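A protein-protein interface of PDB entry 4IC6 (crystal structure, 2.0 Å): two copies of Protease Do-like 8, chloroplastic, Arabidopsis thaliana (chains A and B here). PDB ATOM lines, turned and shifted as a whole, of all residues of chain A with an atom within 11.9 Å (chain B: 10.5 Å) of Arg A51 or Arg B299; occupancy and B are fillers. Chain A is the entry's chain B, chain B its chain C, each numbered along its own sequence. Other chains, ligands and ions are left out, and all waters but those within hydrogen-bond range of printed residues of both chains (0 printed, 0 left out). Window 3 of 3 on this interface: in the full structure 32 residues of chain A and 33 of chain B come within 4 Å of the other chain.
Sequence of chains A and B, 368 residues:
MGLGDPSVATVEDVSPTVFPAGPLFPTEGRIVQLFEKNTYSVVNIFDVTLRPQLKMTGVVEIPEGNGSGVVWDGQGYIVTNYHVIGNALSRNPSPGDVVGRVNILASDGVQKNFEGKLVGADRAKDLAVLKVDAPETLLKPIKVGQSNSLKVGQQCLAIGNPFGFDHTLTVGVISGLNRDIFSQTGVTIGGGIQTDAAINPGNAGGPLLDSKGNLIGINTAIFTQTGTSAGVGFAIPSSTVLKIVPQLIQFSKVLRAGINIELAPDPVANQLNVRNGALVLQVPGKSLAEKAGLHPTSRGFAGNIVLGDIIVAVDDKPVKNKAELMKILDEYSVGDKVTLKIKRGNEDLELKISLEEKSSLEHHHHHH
ND2 of Asn A66 lies close to NE2 of Gln B271.
O of Phe A46 lies within hydrogen-bond range of N of Arg A101 (2.8 Å). N of Asp A47 lies within hydrogen-bond range of OD1 of Asn A66. The side-chain amide oxygen (OE1) of Gln A53 is in hydrogen-bond range of the backbone NH (N) of Lys A55, 2.5 Å away. N of Asn A66 lies within hydrogen-bond range of O of Val A84 (2.8 Å). The backbone NH (N) of Thr B297 sits at hydrogen-bond distance from the backbone carbonyl oxygen (O) of Leu B281, at 2.7 Å. The guanidinium group (NH2) of Arg B299 lies within hydrogen-bond range of the backbone carbonyl oxygen (O) of Gly B303.
CG of Gln B271 touches CD1 of Phe A46, at 3.7 Å. NH1 of Arg B299 touches CB of Arg A51, 3.4 Å away. OE1 of Gln B271 touches CB of Pro A52 (3.6 Å). CG of Pro A52 touches CD2 of Leu B272 (3.7 Å). Val B268 touches Gln A53 (CG2 to O, 3.9 Å). Leu B281 touches Leu A54. Leu B281 touches Lys A55 (CD1 to O, 3.8 Å). Gln B282 touches Lys A55.
Thr A49 touches none of the printed residues of chain B. No residue of chain B comes within 4 Å of Leu A50. Arg A51 touches just one residue of chain B: Arg B299 (3.4 Å). Printed residues of chain B within 4 Å of Pro A52: Gln B271 and Leu B272. Printed residues of chain B within 4 Å of Leu A54: Leu B281. Of the printed residues of chain B, Asn A66 touches Gln B271. Printed residues of chain A within 4 Å of Leu B272: Pro A52 (3.7 Å). Printed residues of chain A within 4 Å of Leu B281: Leu A54 (3.9 Å) and Lys A55 (3.8 Å). No residue of chain A comes within 4 Å of Ser B298. Arg B299 touches one residue of chain A. No residue of chain A comes within 4 Å of Gly B300. No residue of chain A comes within 4 Å of Ala B302. No residue of chain A comes within 4 Å of Gly B303. No residue of chain A comes within 4 Å of Asn B304. The nearest residue of chain B that does not touch Arg A51 is Ile B305 (5.4 Å). The nearest residue of chain A that does not touch Arg B299 is Leu A54 (5.6 Å).
Of the 19 printed residues of chain B, 6 touch a printed residue of chain A. Hydrophobic or aromatic side chains of chain B that line the printed part of chain A: Val B268, Leu B272 and Leu B281. Printed residues of chain A that touch a printed residue of chain B: Phe A46, Arg A51, Pro A52, Gln A53, Leu A54, Lys A55 and Asn A66. Hydrophobic or aromatic side chains of chain A within 4 Å of the printed part of chain B: Phe A46 and Pro A52. Among the printed residues, 9 pairs touch across the chains. Among the printed residues, no Asp or Glu carboxylate lies within 4 Å of a Lys or Arg side-chain nitrogen of the other chain.
No position is printed for both chains. Of the 9 pairs that touch across the chains among the printed residues, none has its exchanged pair printed and touching as well.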
ATOM      1  N   PHE A  46      32.763 -24.616  24.001  1.00  0.00           N
ATOM      2  CA  PHE A  46      31.570 -24.850  24.806  1.00  0.00           C
ATOM      3  C   PHE A  46      31.811 -25.990  25.800  1.00  0.00           C
ATOM      4  O   PHE A  46      32.215 -27.088  25.409  1.00  0.00           O
ATOM      5  CB  PHE A  46      30.358 -25.158  23.920  1.00  0.00           C
ATOM      6  CG  PHE A  46      29.875 -23.975  23.116  1.00  0.00           C
ATOM      7  CD1 PHE A  46      29.441 -22.817  23.751  1.00  0.00           C
ATOM      8  CD2 PHE A  46      29.852 -24.019  21.725  1.00  0.00           C
ATOM      9  CE1 PHE A  46      28.998 -21.714  23.009  1.00  0.00           C
ATOM     10  CE2 PHE A  46      29.403 -22.926  20.978  1.00  0.00           C
ATOM     11  CZ  PHE A  46      28.975 -21.775  21.621  1.00  0.00           C
ATOM     12  N   ASP A  47      31.561 -25.722  27.081  1.00  0.00           N
ATOM     13  CA  ASP A  47      31.672 -26.732  28.141  1.00  0.00           C
ATOM     14  C   ASP A  47      30.530 -27.734  27.992  1.00  0.00           C
ATOM     15  O   ASP A  47      29.369 -27.406  28.254  1.00  0.00           O
ATOM     16  CB  ASP A  47      31.621 -26.050  29.509  1.00  0.00           C
ATOM     17  CG  ASP A  47      31.804 -27.022  30.665  1.00  0.00           C
ATOM     18  OD1 ASP A  47      31.172 -28.103  30.654  1.00  0.00           O
ATOM     19  OD2 ASP A  47      32.579 -26.699  31.596  1.00  0.00           O
ATOM     20  N   VAL A  48      30.853 -28.952  27.568  1.00  0.00           N
ATOM     21  CA  VAL A  48      29.823 -29.929  27.217  1.00  0.00           C
ATOM     22  C   VAL A  48      28.970 -30.388  28.401  1.00  0.00           C
ATOM     23  O   VAL A  48      27.969 -31.079  28.207  1.00  0.00           O
ATOM     24  CB  VAL A  48      30.418 -31.185  26.538  1.00  0.00           C
ATOM     25  CG1 VAL A  48      31.533 -30.801  25.579  1.00  0.00           C
ATOM     26  CG2 VAL A  48      30.928 -32.169  27.585  1.00  0.00           C
ATOM     27  N   THR A  49      29.360 -30.018  29.620  1.00  0.00           N
ATOM     28  CA  THR A  49      28.629 -30.471  30.808  1.00  0.00           C
ATOM     29  C   THR A  49      27.451 -29.559  31.111  1.00  0.00           C
ATOM     30  O   THR A  49      26.652 -29.836  32.006  1.00  0.00           O
ATOM     31  CB  THR A  49      29.528 -30.573  32.067  1.00  0.00           C
ATOM     32  OG1 THR A  49      29.906 -29.263  32.510  1.00  0.00           O
ATOM     33  CG2 THR A  49      30.773 -31.407  31.779  1.00  0.00           C
ATOM     34  N   LEU A  50      27.351 -28.472  30.359  1.00  0.00           N
ATOM     35  CA  LEU A  50      26.290 -27.503  30.561  1.00  0.00           C
ATOM     36  C   LEU A  50      25.100 -27.802  29.657  1.00  0.00           C
ATOM     37  O   LEU A  50      25.197 -27.675  28.436  1.00  0.00           O
ATOM     38  CB  LEU A  50      26.805 -26.093  30.277  1.00  0.00           C
ATOM     39  CG  LEU A  50      27.933 -25.571  31.169  1.00  0.00           C
ATOM     40  CD1 LEU A  50      28.439 -24.228  30.654  1.00  0.00           C
ATOM     41  CD2 LEU A  50      27.468 -25.458  32.610  1.00  0.00           C
ATOM     42  N   ARG A  51      23.986 -28.216  30.256  1.00  0.00           N
ATOM     43  CA  ARG A  51      22.722 -28.273  29.533  1.00  0.00           C
ATOM     44  C   ARG A  51      22.255 -26.831  29.313  1.00  0.00           C
ATOM     45  O   ARG A  51      21.948 -26.120  30.276  1.00  0.00           O
ATOM     46  CB  ARG A  51      21.691 -29.059  30.320  1.00  0.00           C
ATOM     47  N   PRO A  52      22.215 -26.384  28.044  1.00  0.00           N
ATOM     48  CA  PRO A  52      21.848 -24.995  27.734  1.00  0.00           C
ATOM     49  C   PRO A  52      20.377 -24.726  28.047  1.00  0.00           C
ATOM     50  O   PRO A  52      19.682 -25.619  28.542  1.00  0.00           O
ATOM     51  CB  PRO A  52      22.074 -24.897  26.220  1.00  0.00           C
ATOM     52  CG  PRO A  52      22.938 -26.071  25.870  1.00  0.00           C
ATOM     53  CD  PRO A  52      22.544 -27.146  26.829  1.00  0.00           C
ATOM     54  N   GLN A  53      19.914 -23.508  27.773  1.00  0.00           N
ATOM     55  CA  GLN A  53      18.487 -23.209  27.869  1.00  0.00           C
ATOM     56  C   GLN A  53      17.845 -23.341  26.488  1.00  0.00           C
ATOM     57  O   GLN A  53      17.904 -22.412  25.678  1.00  0.00           O
ATOM     58  CB  GLN A  53      18.251 -21.809  28.445  1.00  0.00           C
ATOM     59  CG  GLN A  53      16.863 -21.604  29.054  1.00  0.00           C
ATOM     60  CD  GLN A  53      15.930 -22.784  28.814  1.00  0.00           C
ATOM     61  OE1 GLN A  53      15.124 -22.770  27.884  1.00  0.00           O
ATOM     62  NE2 GLN A  53      16.030 -23.806  29.664  1.00  0.00           N
ATOM     63  N   LEU A  54      17.228 -24.496  26.234  1.00  0.00           N
ATOM     64  CA  LEU A  54      16.693 -24.819  24.911  1.00  0.00           C
ATOM     65  C   LEU A  54      15.266 -24.301  24.684  1.00  0.00           C
ATOM     66  O   LEU A  54      14.520 -24.843  23.860  1.00  0.00           O
ATOM     67  CB  LEU A  54      16.762 -26.321  24.665  1.00  0.00           C
ATOM     68  N   LYS A  55      14.899 -23.252  25.418  1.00  0.00           N
ATOM     69  CA  LYS A  55      13.657 -22.514  25.182  1.00  0.00           C
ATOM     70  C   LYS A  55      13.822 -21.045  25.572  1.00  0.00           C
ATOM     71  O   LYS A  55      13.785 -20.169  24.710  1.00  0.00           O
ATOM     72  CB  LYS A  55      12.489 -23.148  25.950  1.00  0.00           C
ATOM     73  N   GLY A  65      30.431 -20.723  32.325  1.00  0.00           N
ATOM     74  CA  GLY A  65      31.411 -21.295  31.418  1.00  0.00           C
ATOM     75  C   GLY A  65      31.286 -20.843  29.963  1.00  0.00           C
ATOM     76  O   GLY A  65      30.512 -19.937  29.638  1.00  0.00           O
ATOM     77  N   ASN A  66      32.061 -21.491  29.090  1.00  0.00           N
ATOM     78  CA  ASN A  66      32.077 -21.212  27.650  1.00  0.00           C
ATOM     79  C   ASN A  66      32.800 -19.928  27.332  1.00  0.00           C
ATOM     80  O   ASN A  66      32.748 -18.978  28.104  1.00  0.00           O
ATOM     81  CB  ASN A  66      30.663 -21.142  27.081  1.00  0.00           C
ATOM     82  CG  ASN A  66      29.777 -22.238  27.615  1.00  0.00           C
ATOM     83  OD1 ASN A  66      30.265 -23.257  28.108  1.00  0.00           O
ATOM     84  ND2 ASN A  66      28.467 -22.039  27.530  1.00  0.00           N
ATOM     85  N   VAL A  84      36.726 -21.242  31.747  1.00  0.00           N
ATOM     86  CA  VAL A  84      35.756 -21.422  30.653  1.00  0.00           C
ATOM     87  C   VAL A  84      35.245 -22.873  30.585  1.00  0.00           C
ATOM     88  O   VAL A  84      34.156 -23.142  30.079  1.00  0.00           O
ATOM     89  CB  VAL A  84      36.203 -20.849  29.271  1.00  0.00           C
ATOM     90  CG1 VAL A  84      37.176 -19.681  29.446  1.00  0.00           C
ATOM     91  CG2 VAL A  84      36.758 -21.917  28.363  1.00  0.00           C
ATOM     92  N   GLY A  86      35.200 -24.531  33.622  1.00  0.00           N
ATOM     93  CA  GLY A  86      35.133 -24.691  35.062  1.00  0.00           C
ATOM     94  C   GLY A  86      34.162 -25.754  35.522  1.00  0.00           C
ATOM     95  O   GLY A  86      34.515 -26.605  36.338  1.00  0.00           O
ATOM     96  N   ASN A  87      32.935 -25.720  35.010  1.00  0.00           N
ATOM     97  CA  ASN A  87      31.936 -26.685  35.449  1.00  0.00           C
ATOM     98  C   ASN A  87      32.371 -28.112  35.142  1.00  0.00           C
ATOM     99  O   ASN A  87      32.200 -29.016  35.965  1.00  0.00           O
ATOM    100  CB  ASN A  87      30.565 -26.393  34.840  1.00  0.00           C
ATOM    101  CG  ASN A  87      29.449 -27.145  35.541  1.00  0.00           C
ATOM    102  OD1 ASN A  87      29.036 -26.780  36.644  1.00  0.00           O
ATOM    103  ND2 ASN A  87      28.958 -28.203  34.906  1.00  0.00           N
ATOM    104  N   ALA A  88      32.952 -28.310  33.963  1.00  0.00           N
ATOM    105  CA  ALA A  88      33.435 -29.633  33.573  1.00  0.00           C
ATOM    106  C   ALA A  88      34.602 -30.110  34.450  1.00  0.00           C
ATOM    107  O   ALA A  88      34.668 -31.281  34.836  1.00  0.00           O
ATOM    108  CB  ALA A  88      33.825 -29.640  32.112  1.00  0.00           C
ATOM    109  N   SER A  90      35.048 -29.292  37.402  1.00  0.00           N
ATOM    110  CA  SER A  90      34.498 -29.502  38.741  1.00  0.00           C
ATOM    111  C   SER A  90      34.025 -30.939  38.902  1.00  0.00           C
ATOM    112  O   SER A  90      33.634 -31.357  39.999  1.00  0.00           O
ATOM    113  CB  SER A  90      33.320 -28.563  39.005  1.00  0.00           C
ATOM    114  OG  SER A  90      32.100 -29.170  38.611  1.00  0.00           O
ATOM    115  N   ARG A  91      34.050 -31.696  37.809  1.00  0.00           N
ATOM    116  CA  ARG A  91      33.606 -33.082  37.853  1.00  0.00           C
ATOM    117  C   ARG A  91      34.766 -34.073  37.816  1.00  0.00           C
ATOM    118  O   ARG A  91      34.582 -35.248  37.487  1.00  0.00           O
ATOM    119  CB  ARG A  91      32.597 -33.364  36.744  1.00  0.00           C
ATOM    120  CG  ARG A  91      31.357 -32.497  36.845  1.00  0.00           C
ATOM    121  CD  ARG A  91      30.319 -32.905  35.834  1.00  0.00           C
ATOM    122  NE  ARG A  91      29.119 -32.080  35.932  1.00  0.00           N
ATOM    123  CZ  ARG A  91      28.033 -32.268  35.191  1.00  0.00           C
ATOM    124  NH1 ARG A  91      28.005 -33.255  34.306  1.00  0.00           N
ATOM    125  NH2 ARG A  91      26.979 -31.473  35.334  1.00  0.00           N
ATOM    126  N   VAL A  99      35.881 -32.839  27.107  1.00  0.00           N
ATOM    127  CA  VAL A  99      35.475 -31.875  28.112  1.00  0.00           C
ATOM    128  C   VAL A  99      34.973 -30.580  27.469  1.00  0.00           C
ATOM    129  O   VAL A  99      34.358 -29.727  28.120  1.00  0.00           O
ATOM    130  CB  VAL A  99      36.629 -31.651  29.108  1.00  0.00           C
ATOM    131  CG1 VAL A  99      37.702 -30.755  28.521  1.00  0.00           C
ATOM    132  CG2 VAL A  99      36.109 -31.118  30.425  1.00  0.00           C
ATOM    133  N   GLY A 100      35.202 -30.448  26.170  1.00  0.00           N
ATOM    134  CA  GLY A 100      34.760 -29.262  25.460  1.00  0.00           C
ATOM    135  C   GLY A 100      34.405 -29.535  24.017  1.00  0.00           C
ATOM    136  O   GLY A 100      34.841 -30.530  23.429  1.00  0.00           O
ATOM    137  N   ARG A 101      33.578 -28.655  23.463  1.00  0.00           N
ATOM    138  CA  ARG A 101      33.308 -28.605  22.037  1.00  0.00           C
ATOM    139  C   ARG A 101      34.094 -27.422  21.516  1.00  0.00           C
ATOM    140  O   ARG A 101      33.974 -26.320  22.040  1.00  0.00           O
ATOM    141  CB  ARG A 101      31.817 -28.368  21.774  1.00  0.00           C
ATOM    142  CG  ARG A 101      31.015 -29.616  21.586  1.00  0.00           C
ATOM    143  CD  ARG A 101      31.740 -30.546  20.633  1.00  0.00           C
ATOM    144  NE  ARG A 101      30.933 -31.693  20.231  1.00  0.00           N
ATOM    145  CZ  ARG A 101      31.309 -32.566  19.304  1.00  0.00           C
ATOM    146  NH1 ARG A 101      32.477 -32.418  18.694  1.00  0.00           N
ATOM    147  NH2 ARG A 101      30.522 -33.583  18.987  1.00  0.00           N
ATOM    148  N   VAL B 268      22.608 -19.371  21.543  1.00  0.00           N
ATOM    149  CA  VAL B 268      21.925 -20.603  21.915  1.00  0.00           C
ATOM    150  C   VAL B 268      21.979 -21.651  20.805  1.00  0.00           C
ATOM    151  O   VAL B 268      22.168 -22.842  21.071  1.00  0.00           O
ATOM    152  CB  VAL B 268      20.450 -20.348  22.295  1.00  0.00           C
ATOM    153  CG1 VAL B 268      19.584 -21.542  21.915  1.00  0.00           C
ATOM    154  CG2 VAL B 268      20.328 -20.050  23.779  1.00  0.00           C
ATOM    155  N   GLN B 271      25.306 -23.201  20.384  1.00  0.00           N
ATOM    156  CA  GLN B 271      25.639 -24.006  21.552  1.00  0.00           C
ATOM    157  C   GLN B 271      25.127 -25.418  21.298  1.00  0.00           C
ATOM    158  O   GLN B 271      25.685 -26.407  21.782  1.00  0.00           O
ATOM    159  CB  GLN B 271      24.976 -23.424  22.801  1.00  0.00           C
ATOM    160  CG  GLN B 271      25.833 -23.475  24.059  1.00  0.00           C
ATOM    161  CD  GLN B 271      25.123 -22.902  25.276  1.00  0.00           C
ATOM    162  OE1 GLN B 271      24.172 -22.128  25.150  1.00  0.00           O
ATOM    163  NE2 GLN B 271      25.580 -23.292  26.466  1.00  0.00           N
ATOM    164  N   LEU B 272      24.052 -25.487  20.521  1.00  0.00           N
ATOM    165  CA  LEU B 272      23.419 -26.745  20.159  1.00  0.00           C
ATOM    166  C   LEU B 272      23.959 -27.263  18.838  1.00  0.00           C
ATOM    167  O   LEU B 272      23.360 -28.128  18.202  1.00  0.00           O
ATOM    168  CB  LEU B 272      21.907 -26.555  20.064  1.00  0.00           C
ATOM    169  CG  LEU B 272      21.279 -26.206  21.404  1.00  0.00           C
ATOM    170  CD1 LEU B 272      19.774 -26.337  21.309  1.00  0.00           C
ATOM    171  CD2 LEU B 272      21.839 -27.138  22.483  1.00  0.00           C
ATOM    172  N   VAL B 280      14.223 -23.564  14.978  1.00  0.00           N
ATOM    173  CA  VAL B 280      12.909 -23.398  15.579  1.00  0.00           C
ATOM    174  C   VAL B 280      12.897 -23.981  16.990  1.00  0.00           C
ATOM    175  O   VAL B 280      13.107 -25.183  17.166  1.00  0.00           O
ATOM    176  CB  VAL B 280      11.836 -24.125  14.762  1.00  0.00           C
ATOM    177  CG1 VAL B 280      10.487 -24.033  15.465  1.00  0.00           C
ATOM    178  CG2 VAL B 280      11.757 -23.563  13.354  1.00  0.00           C
ATOM    179  N   LEU B 281      12.650 -23.140  17.990  1.00  0.00           N
ATOM    180  CA  LEU B 281      12.536 -23.623  19.364  1.00  0.00           C
ATOM    181  C   LEU B 281      11.090 -23.976  19.736  1.00  0.00           C
ATOM    182  O   LEU B 281      10.756 -25.149  19.876  1.00  0.00           O
ATOM    183  CB  LEU B 281      13.113 -22.616  20.359  1.00  0.00           C
ATOM    184  CG  LEU B 281      14.605 -22.288  20.223  1.00  0.00           C
ATOM    185  CD1 LEU B 281      15.027 -21.279  21.276  1.00  0.00           C
ATOM    186  CD2 LEU B 281      15.451 -23.557  20.324  1.00  0.00           C
ATOM    187  N   GLN B 282      10.241 -22.962  19.893  1.00  0.00           N
ATOM    188  CA  GLN B 282       8.858 -23.169  20.333  1.00  0.00           C
ATOM    189  C   GLN B 282       7.853 -23.052  19.185  1.00  0.00           C
ATOM    190  O   GLN B 282       8.044 -22.263  18.255  1.00  0.00           O
ATOM    191  CB  GLN B 282       8.495 -22.159  21.426  1.00  0.00           C
ATOM    192  CG  GLN B 282       9.347 -22.239  22.684  1.00  0.00           C
ATOM    193  CD  GLN B 282       9.244 -20.981  23.536  1.00  0.00           C
ATOM    194  OE1 GLN B 282       9.041 -19.881  23.016  1.00  0.00           O
ATOM    195  NE2 GLN B 282       9.383 -21.139  24.851  1.00  0.00           N
ATOM    196  N   PRO B 296       8.948 -28.177  16.938  1.00  0.00           N
ATOM    197  CA  PRO B 296       9.701 -27.455  17.973  1.00  0.00           C
ATOM    198  C   PRO B 296      10.916 -28.250  18.460  1.00  0.00           C
ATOM    199  O   PRO B 296      11.141 -29.373  18.015  1.00  0.00           O
ATOM    200  CB  PRO B 296       8.682 -27.327  19.107  1.00  0.00           C
ATOM    201  CG  PRO B 296       7.805 -28.526  18.944  1.00  0.00           C
ATOM    202  CD  PRO B 296       7.689 -28.740  17.457  1.00  0.00           C
ATOM    203  N   THR B 297      11.695 -27.661  19.362  1.00  0.00           N
ATOM    204  CA  THR B 297      12.841 -28.347  19.953  1.00  0.00           C
ATOM    205  C   THR B 297      12.436 -28.928  21.311  1.00  0.00           C
ATOM    206  O   THR B 297      11.771 -28.254  22.101  1.00  0.00           O
ATOM    207  CB  THR B 297      14.045 -27.394  20.118  1.00  0.00           C
ATOM    208  OG1 THR B 297      14.397 -26.839  18.844  1.00  0.00           O
ATOM    209  CG2 THR B 297      15.242 -28.134  20.688  1.00  0.00           C
ATOM    210  N   SER B 298      12.829 -30.171  21.583  1.00  0.00           N
ATOM    211  CA  SER B 298      12.360 -30.859  22.787  1.00  0.00           C
ATOM    212  C   SER B 298      13.462 -31.560  23.583  1.00  0.00           C
ATOM    213  O   SER B 298      14.226 -32.359  23.035  1.00  0.00           O
ATOM    214  CB  SER B 298      11.251 -31.853  22.437  1.00  0.00           C
ATOM    215  N   ARG B 299      13.525 -31.261  24.879  1.00  0.00           N
ATOM    216  CA  ARG B 299      14.348 -32.027  25.812  1.00  0.00           C
ATOM    217  C   ARG B 299      13.518 -33.138  26.455  1.00  0.00           C
ATOM    218  O   ARG B 299      12.593 -32.867  27.220  1.00  0.00           O
ATOM    219  CB  ARG B 299      14.954 -31.116  26.885  1.00  0.00           C
ATOM    220  CG  ARG B 299      15.317 -31.853  28.168  1.00  0.00           C
ATOM    221  CD  ARG B 299      16.506 -31.225  28.882  1.00  0.00           C
ATOM    222  NE  ARG B 299      17.554 -32.216  29.124  1.00  0.00           N
ATOM    223  CZ  ARG B 299      18.622 -32.022  29.893  1.00  0.00           C
ATOM    224  NH1 ARG B 299      18.799 -30.866  30.520  1.00  0.00           N
ATOM    225  NH2 ARG B 299      19.514 -32.992  30.039  1.00  0.00           N
ATOM    226  N   GLY B 300      13.845 -34.386  26.130  1.00  0.00           N
ATOM    227  CA  GLY B 300      13.139 -35.532  26.679  1.00  0.00           C
ATOM    228  C   GLY B 300      13.551 -35.781  28.115  1.00  0.00           C
ATOM    229  O   GLY B 300      14.624 -35.350  28.536  1.00  0.00           O
ATOM    230  N   PHE B 301      12.701 -36.463  28.874  1.00  0.00           N
ATOM    231  CA  PHE B 301      12.989 -36.732  30.277  1.00  0.00           C
ATOM    232  C   PHE B 301      14.249 -37.574  30.423  1.00  0.00           C
ATOM    233  O   PHE B 301      14.986 -37.442  31.403  1.00  0.00           O
ATOM    234  CB  PHE B 301      11.805 -37.432  30.956  1.00  0.00           C
ATOM    235  CG  PHE B 301      11.940 -37.540  32.451  1.00  0.00           C
ATOM    236  CD1 PHE B 301      12.148 -38.766  33.055  1.00  0.00           C
ATOM    237  CD2 PHE B 301      11.870 -36.406  33.252  1.00  0.00           C
ATOM    238  CE1 PHE B 301      12.273 -38.865  34.431  1.00  0.00           C
ATOM    239  CE2 PHE B 301      11.993 -36.500  34.632  1.00  0.00           C
ATOM    240  CZ  PHE B 301      12.196 -37.728  35.219  1.00  0.00           C
ATOM    241  N   ALA B 302      14.492 -38.444  29.447  1.00  0.00           N
ATOM    242  CA  ALA B 302      15.668 -39.300  29.479  1.00  0.00           C
ATOM    243  C   ALA B 302      16.937 -38.475  29.266  1.00  0.00           C
ATOM    244  O   ALA B 302      17.908 -38.954  28.685  1.00  0.00           O
ATOM    245  CB  ALA B 302      15.557 -40.404  28.441  1.00  0.00           C
ATOM    246  N   GLY B 303      16.914 -37.231  29.733  1.00  0.00           N
ATOM    247  CA  GLY B 303      18.083 -36.371  29.709  1.00  0.00           C
ATOM    248  C   GLY B 303      18.458 -35.762  28.366  1.00  0.00           C
ATOM    249  O   GLY B 303      19.312 -34.877  28.306  1.00  0.00           O
ATOM    250  N   ASN B 304      17.818 -36.210  27.292  1.00  0.00           N
ATOM    251  CA  ASN B 304      18.268 -35.872  25.941  1.00  0.00           C
ATOM    252  C   ASN B 304      17.670 -34.605  25.331  1.00  0.00           C
ATOM    253  O   ASN B 304      16.616 -34.134  25.756  1.00  0.00           O
ATOM    254  CB  ASN B 304      17.968 -37.035  25.004  1.00  0.00           C
ATOM    255  CG  ASN B 304      16.482 -37.283  24.853  1.00  0.00           C
ATOM    256  OD1 ASN B 304      15.832 -37.799  25.765  1.00  0.00           O
ATOM    257  ND2 ASN B 304      15.932 -36.911  23.700  1.00  0.00           N
ATOM    258  N   ILE B 305      18.354 -34.081  24.315  1.00  0.00           N
ATOM    259  CA  ILE B 305      17.849 -32.981  23.493  1.00  0.00           C
ATOM    260  C   ILE B 305      17.543 -33.458  22.070  1.00  0.00           C
ATOM    261  O   ILE B 305      18.358 -34.136  21.448  1.00  0.00           O
ATOM    262  CB  ILE B 305      18.868 -31.831  23.399  1.00  0.00           C
ATOM    263  CG1 ILE B 305      18.665 -30.836  24.541  1.00  0.00           C
ATOM    264  CG2 ILE B 305      18.746 -31.110  22.062  1.00  0.00           C
ATOM    265  CD1 ILE B 305      19.832 -30.761  25.497  1.00  0.00           C
ATOM    266  N   VAL B 306      16.368 -33.104  21.559  1.00  0.00           N
ATOM    267  CA  VAL B 306      16.026 -33.391  20.168  1.00  0.00           C
ATOM    268  C   VAL B 306      15.687 -32.092  19.430  1.00  0.00           C
ATOM    269  O   VAL B 306      14.905 -31.275  19.920  1.00  0.00           O
ATOM    270  CB  VAL B 306      14.879 -34.414  20.062  1.00  0.00           C
ATOM    271  CG1 VAL B 306      14.162 -34.272  18.728  1.00  0.00           C
ATOM    272  CG2 VAL B 306      15.416 -35.841  20.256  1.00  0.00           C
ATOM    273  N   LEU B 307      16.280 -31.907  18.254  1.00  0.00           N
ATOM    274  CA  LEU B 307      16.259 -30.606  17.589  1.00  0.00           C
ATOM    275  C   LEU B 307      14.993 -30.266  16.813  1.00  0.00           C
ATOM    276  O   LEU B 307      14.526 -31.043  15.973  1.00  0.00           O
ATOM    277  CB  LEU B 307      17.465 -30.448  16.664  1.00  0.00           C
ATOM    278  CG  LEU B 307      18.730 -29.898  17.312  1.00  0.00           C
ATOM    279  CD1 LEU B 307      19.671 -29.443  16.225  1.00  0.00           C
ATOM    280  CD2 LEU B 307      18.391 -28.747  18.245  1.00  0.00           C
ATOM    281  N   GLY B 308      14.457 -29.083  17.092  1.00  0.00           N
ATOM    282  CA  GLY B 308      13.369 -28.548  16.302  1.00  0.00           C
ATOM    283  C   GLY B 308      13.850 -28.368  14.878  1.00  0.00           C
ATOM    284  O   GLY B 308      15.058 -28.389  14.622  1.00  0.00           O
